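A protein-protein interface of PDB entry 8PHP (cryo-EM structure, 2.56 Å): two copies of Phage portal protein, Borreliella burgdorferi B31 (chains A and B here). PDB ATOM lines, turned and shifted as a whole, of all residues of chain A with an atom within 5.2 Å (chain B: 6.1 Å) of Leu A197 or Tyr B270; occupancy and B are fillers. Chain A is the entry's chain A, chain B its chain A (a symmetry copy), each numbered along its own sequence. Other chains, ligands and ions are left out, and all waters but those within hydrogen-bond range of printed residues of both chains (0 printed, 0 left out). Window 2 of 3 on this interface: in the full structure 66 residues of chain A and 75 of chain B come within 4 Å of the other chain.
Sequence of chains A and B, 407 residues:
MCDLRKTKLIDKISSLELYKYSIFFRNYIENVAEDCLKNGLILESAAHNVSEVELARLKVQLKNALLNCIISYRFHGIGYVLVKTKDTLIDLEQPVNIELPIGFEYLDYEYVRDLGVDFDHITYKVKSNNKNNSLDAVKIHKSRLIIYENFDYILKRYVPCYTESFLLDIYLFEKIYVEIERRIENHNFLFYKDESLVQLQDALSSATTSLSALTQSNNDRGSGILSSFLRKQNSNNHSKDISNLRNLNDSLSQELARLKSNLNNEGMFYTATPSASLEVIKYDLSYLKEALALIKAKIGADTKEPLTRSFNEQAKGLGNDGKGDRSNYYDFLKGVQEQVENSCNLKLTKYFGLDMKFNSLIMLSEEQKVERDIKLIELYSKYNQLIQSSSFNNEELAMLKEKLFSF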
ATOM      1  N   TYR A 192     -20.247 -30.938 -27.379  1.00  0.00           N
ATOM      2  CA  TYR A 192     -20.050 -29.524 -27.667  1.00  0.00           C
ATOM      3  C   TYR A 192     -18.848 -29.002 -26.893  1.00  0.00           C
ATOM      4  O   TYR A 192     -18.764 -29.181 -25.673  1.00  0.00           O
ATOM      5  CB  TYR A 192     -21.303 -28.722 -27.310  1.00  0.00           C
ATOM      6  CG  TYR A 192     -21.219 -27.251 -27.646  1.00  0.00           C
ATOM      7  CD1 TYR A 192     -20.666 -26.823 -28.844  1.00  0.00           C
ATOM      8  CD2 TYR A 192     -21.703 -26.292 -26.768  1.00  0.00           C
ATOM      9  CE1 TYR A 192     -20.591 -25.479 -29.155  1.00  0.00           C
ATOM     10  CE2 TYR A 192     -21.633 -24.948 -27.071  1.00  0.00           C
ATOM     11  CZ  TYR A 192     -21.077 -24.547 -28.266  1.00  0.00           C
ATOM     12  OH  TYR A 192     -21.006 -23.208 -28.570  1.00  0.00           O
ATOM     13  N   LYS A 193     -17.925 -28.356 -27.603  1.00  0.00           N
ATOM     14  CA  LYS A 193     -16.751 -27.735 -27.005  1.00  0.00           C
ATOM     15  C   LYS A 193     -16.802 -26.241 -27.285  1.00  0.00           C
ATOM     16  O   LYS A 193     -16.870 -25.828 -28.447  1.00  0.00           O
ATOM     17  CB  LYS A 193     -15.461 -28.341 -27.560  1.00  0.00           C
ATOM     18  CG  LYS A 193     -15.342 -29.840 -27.360  1.00  0.00           C
ATOM     19  CD  LYS A 193     -13.900 -30.300 -27.484  1.00  0.00           C
ATOM     20  CE  LYS A 193     -13.313 -29.924 -28.833  1.00  0.00           C
ATOM     21  NZ  LYS A 193     -11.891 -30.345 -28.954  1.00  0.00           N
ATOM     22  N   ASP A 194     -16.767 -25.436 -26.225  1.00  0.00           N
ATOM     23  CA  ASP A 194     -16.829 -23.984 -26.375  1.00  0.00           C
ATOM     24  C   ASP A 194     -16.187 -23.358 -25.146  1.00  0.00           C
ATOM     25  O   ASP A 194     -16.755 -23.422 -24.051  1.00  0.00           O
ATOM     26  CB  ASP A 194     -18.270 -23.519 -26.545  1.00  0.00           C
ATOM     27  CG  ASP A 194     -18.367 -22.111 -27.098  1.00  0.00           C
ATOM     28  OD1 ASP A 194     -17.313 -21.475 -27.296  1.00  0.00           O
ATOM     29  OD2 ASP A 194     -19.500 -21.643 -27.337  1.00  0.00           O
ATOM     30  N   GLU A 195     -15.011 -22.754 -25.328  1.00  0.00           N
ATOM     31  CA  GLU A 195     -14.302 -22.163 -24.198  1.00  0.00           C
ATOM     32  C   GLU A 195     -14.952 -20.859 -23.751  1.00  0.00           C
ATOM     33  O   GLU A 195     -15.013 -20.571 -22.550  1.00  0.00           O
ATOM     34  CB  GLU A 195     -12.836 -21.935 -24.561  1.00  0.00           C
ATOM     35  CG  GLU A 195     -12.623 -21.404 -25.967  1.00  0.00           C
ATOM     36  CD  GLU A 195     -11.156 -21.244 -26.312  1.00  0.00           C
ATOM     37  OE1 GLU A 195     -10.306 -21.492 -25.432  1.00  0.00           O
ATOM     38  OE2 GLU A 195     -10.853 -20.871 -27.465  1.00  0.00           O
ATOM     39  N   SER A 196     -15.442 -20.057 -24.699  1.00  0.00           N
ATOM     40  CA  SER A 196     -16.026 -18.768 -24.345  1.00  0.00           C
ATOM     41  C   SER A 196     -17.344 -18.937 -23.599  1.00  0.00           C
ATOM     42  O   SER A 196     -17.649 -18.163 -22.683  1.00  0.00           O
ATOM     43  CB  SER A 196     -16.226 -17.920 -25.599  1.00  0.00           C
ATOM     44  OG  SER A 196     -15.034 -17.852 -26.361  1.00  0.00           O
ATOM     45  N   LEU A 197     -18.136 -19.936 -23.971  1.00  0.00           N
ATOM     46  CA  LEU A 197     -19.426 -20.167 -23.330  1.00  0.00           C
ATOM     47  C   LEU A 197     -19.247 -20.677 -21.904  1.00  0.00           C
ATOM     48  O   LEU A 197     -19.860 -20.163 -20.969  1.00  0.00           O
ATOM     49  CB  LEU A 197     -20.258 -21.159 -24.142  1.00  0.00           C
ATOM     50  CG  LEU A 197     -21.675 -21.423 -23.632  1.00  0.00           C
ATOM     51  CD1 LEU A 197     -22.517 -20.158 -23.703  1.00  0.00           C
ATOM     52  CD2 LEU A 197     -22.325 -22.550 -24.416  1.00  0.00           C
ATOM     53  N   LEU A 259     -29.456 -21.966 -26.201  1.00  0.00           N
ATOM     54  CA  LEU A 259     -29.007 -22.741 -27.353  1.00  0.00           C
ATOM     55  C   LEU A 259     -30.109 -23.658 -27.870  1.00  0.00           C
ATOM     56  O   LEU A 259     -30.314 -23.771 -29.084  1.00  0.00           O
ATOM     57  CB  LEU A 259     -27.764 -23.551 -26.984  1.00  0.00           C
ATOM     58  CG  LEU A 259     -26.508 -22.746 -26.647  1.00  0.00           C
ATOM     59  CD1 LEU A 259     -25.352 -23.675 -26.313  1.00  0.00           C
ATOM     60  CD2 LEU A 259     -26.141 -21.815 -27.791  1.00  0.00           C
ATOM     61  N   THR A 273     -17.049 -18.566 -31.073  1.00  0.00           N
ATOM     62  CA  THR A 273     -15.689 -19.038 -30.840  1.00  0.00           C
ATOM     63  C   THR A 273     -15.144 -19.690 -32.102  1.00  0.00           C
ATOM     64  O   THR A 273     -15.771 -20.620 -32.627  1.00  0.00           O
ATOM     65  CB  THR A 273     -15.661 -20.027 -29.681  1.00  0.00           C
ATOM     66  OG1 THR A 273     -16.094 -19.373 -28.482  1.00  0.00           O
ATOM     67  CG2 THR A 273     -14.256 -20.566 -29.475  1.00  0.00           C
ATOM     68  N   TYR B 192     -12.921 -40.538 -22.368  1.00  0.00           N
ATOM     69  CA  TYR B 192     -12.997 -39.096 -22.175  1.00  0.00           C
ATOM     70  C   TYR B 192     -11.658 -38.572 -21.676  1.00  0.00           C
ATOM     71  O   TYR B 192     -11.113 -39.083 -20.692  1.00  0.00           O
ATOM     72  CB  TYR B 192     -14.109 -38.743 -21.187  1.00  0.00           C
ATOM     73  CG  TYR B 192     -14.312 -37.260 -20.980  1.00  0.00           C
ATOM     74  CD1 TYR B 192     -14.287 -36.379 -22.052  1.00  0.00           C
ATOM     75  CD2 TYR B 192     -14.540 -36.742 -19.713  1.00  0.00           C
ATOM     76  CE1 TYR B 192     -14.476 -35.024 -21.868  1.00  0.00           C
ATOM     77  CE2 TYR B 192     -14.731 -35.389 -19.519  1.00  0.00           C
ATOM     78  CZ  TYR B 192     -14.699 -34.535 -20.600  1.00  0.00           C
ATOM     79  OH  TYR B 192     -14.888 -33.187 -20.409  1.00  0.00           O
ATOM     80  N   LEU B 259     -21.958 -34.654 -15.269  1.00  0.00           N
ATOM     81  CA  LEU B 259     -21.884 -34.927 -16.701  1.00  0.00           C
ATOM     82  C   LEU B 259     -22.993 -35.873 -17.145  1.00  0.00           C
ATOM     83  O   LEU B 259     -23.616 -35.661 -18.193  1.00  0.00           O
ATOM     84  CB  LEU B 259     -20.513 -35.507 -17.050  1.00  0.00           C
ATOM     85  CG  LEU B 259     -19.315 -34.577 -16.851  1.00  0.00           C
ATOM     86  CD1 LEU B 259     -18.025 -35.277 -17.247  1.00  0.00           C
ATOM     87  CD2 LEU B 259     -19.495 -33.290 -17.639  1.00  0.00           C
ATOM     88  N   MET B 268     -26.937 -33.352 -24.287  1.00  0.00           N
ATOM     89  CA  MET B 268     -25.766 -32.646 -24.783  1.00  0.00           C
ATOM     90  C   MET B 268     -24.650 -32.742 -23.756  1.00  0.00           C
ATOM     91  O   MET B 268     -24.871 -32.487 -22.568  1.00  0.00           O
ATOM     92  CB  MET B 268     -26.085 -31.178 -25.080  1.00  0.00           C
ATOM     93  CG  MET B 268     -24.894 -30.375 -25.575  1.00  0.00           C
ATOM     94  SD  MET B 268     -25.297 -28.649 -25.895  1.00  0.00           S
ATOM     95  CE  MET B 268     -26.395 -28.814 -27.301  1.00  0.00           C
ATOM     96  N   PHE B 269     -23.457 -33.111 -24.214  1.00  0.00           N
ATOM     97  CA  PHE B 269     -22.273 -33.179 -23.369  1.00  0.00           C
ATOM     98  C   PHE B 269     -21.412 -31.954 -23.653  1.00  0.00           C
ATOM     99  O   PHE B 269     -20.954 -31.764 -24.784  1.00  0.00           O
ATOM    100  CB  PHE B 269     -21.493 -34.467 -23.630  1.00  0.00           C
ATOM    101  CG  PHE B 269     -20.361 -34.697 -22.673  1.00  0.00           C
ATOM    102  CD1 PHE B 269     -20.598 -35.229 -21.417  1.00  0.00           C
ATOM    103  CD2 PHE B 269     -19.062 -34.381 -23.025  1.00  0.00           C
ATOM    104  CE1 PHE B 269     -19.559 -35.444 -20.535  1.00  0.00           C
ATOM    105  CE2 PHE B 269     -18.019 -34.593 -22.146  1.00  0.00           C
ATOM    106  CZ  PHE B 269     -18.268 -35.125 -20.899  1.00  0.00           C
ATOM    107  N   TYR B 270     -21.195 -31.131 -22.632  1.00  0.00           N
ATOM    108  CA  TYR B 270     -20.515 -29.854 -22.788  1.00  0.00           C
ATOM    109  C   TYR B 270     -19.195 -29.856 -22.029  1.00  0.00           C
ATOM    110  O   TYR B 270     -19.095 -30.423 -20.936  1.00  0.00           O
ATOM    111  CB  TYR B 270     -21.392 -28.700 -22.296  1.00  0.00           C
ATOM    112  CG  TYR B 270     -20.671 -27.374 -22.227  1.00  0.00           C
ATOM    113  CD1 TYR B 270     -20.312 -26.697 -23.384  1.00  0.00           C
ATOM    114  CD2 TYR B 270     -20.342 -26.802 -21.005  1.00  0.00           C
ATOM    115  CE1 TYR B 270     -19.651 -25.485 -23.327  1.00  0.00           C
ATOM    116  CE2 TYR B 270     -19.681 -25.591 -20.939  1.00  0.00           C
ATOM    117  CZ  TYR B 270     -19.338 -24.938 -22.103  1.00  0.00           C
ATOM    118  OH  TYR B 270     -18.680 -23.732 -22.042  1.00  0.00           O
ATOM    119  N   THR B 271     -18.187 -29.216 -22.618  1.00  0.00           N
ATOM    120  CA  THR B 271     -16.897 -29.039 -21.971  1.00  0.00           C
ATOM    121  C   THR B 271     -16.291 -27.727 -22.446  1.00  0.00           C
ATOM    122  O   THR B 271     -16.659 -27.194 -23.496  1.00  0.00           O
ATOM    123  CB  THR B 271     -15.946 -30.207 -22.259  1.00  0.00           C
ATOM    124  OG1 THR B 271     -14.762 -30.066 -21.464  1.00  0.00           O
ATOM    125  CG2 THR B 271     -15.563 -30.235 -23.727  1.00  0.00           C
ATOM    126  N   ALA B 272     -15.356 -27.205 -21.653  1.00  0.00           N
ATOM    127  CA  ALA B 272     -14.710 -25.936 -21.953  1.00  0.00           C
ATOM    128  C   ALA B 272     -13.252 -26.077 -22.363  1.00  0.00           C
ATOM    129  O   ALA B 272     -12.672 -25.106 -22.861  1.00  0.00           O
ATOM    130  CB  ALA B 272     -14.804 -24.992 -20.746  1.00  0.00           C
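The backbone carbonyl oxygen (O) of Asp A194 sits at hydrogen-bond distance from the side-chain hydroxyl (OH) of Tyr B270, 2.8 Å away. The backbone carbonyl oxygen (O) of Tyr A192 lies within hydrogen-bond range of the backbone NH (N) of Thr B271 (3.1 Å). The backbone NH (N) of Tyr A192 is in hydrogen-bond range of the backbone carbonyl oxygen (O) of Phe B269. The backbone NH (N) of Asp A194 is in hydrogen-bond range of the backbone carbonyl oxygen (O) of Thr B271 (3.2 Å).
The side-chain hydroxyl (OG1) of Thr B271 lies within hydrogen-bond range of the side-chain hydroxyl (OH) of Tyr B192 (3.3 Å). The side-chain carboxylate of Asp A194 sits at hydrogen-bond distance from the side-chain hydroxyl of Tyr A192 (2.5 Å). The side-chain carboxylate of Asp A194 lies within hydrogen-bond range of the side-chain hydroxyl of Thr A273 (2.7 Å).
Among the printed residues, merely in contact across the chains: Leu A197 with Tyr B270 (3.1 Å), Tyr A192 with Tyr B270 (3.4 Å), Lys A193 with Thr B271 (3.6 Å), Glu A195 with Ala B272 (3.6 Å) and Asp A194 with Ala B272 (3.9 Å).
Tyr B270 touches just these residues of chain A: Tyr A192, Asp A194 and Leu A197. Of the printed residues of chain A, Ala B272 touches Asp A194 and Glu A195. Of the printed residues of chain B, Tyr A192 touches Phe B269, Tyr B270 and Thr B271.
Hydrophobic or aromatic side chains of chain B within 4 Å of the printed part of chain A: Tyr B270. Hydrophobic or aromatic side chains of chain A that line the printed part of chain B: Tyr A192 and Leu A197. Along chain A the printed residues that touch a printed residue of chain B span positions 192 to 197. Among the printed residues, no Asp or Glu carboxylate lies within 4 Å of a Lys or Arg side-chain nitrogen of the other chain.
2 positions are printed for both chains.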
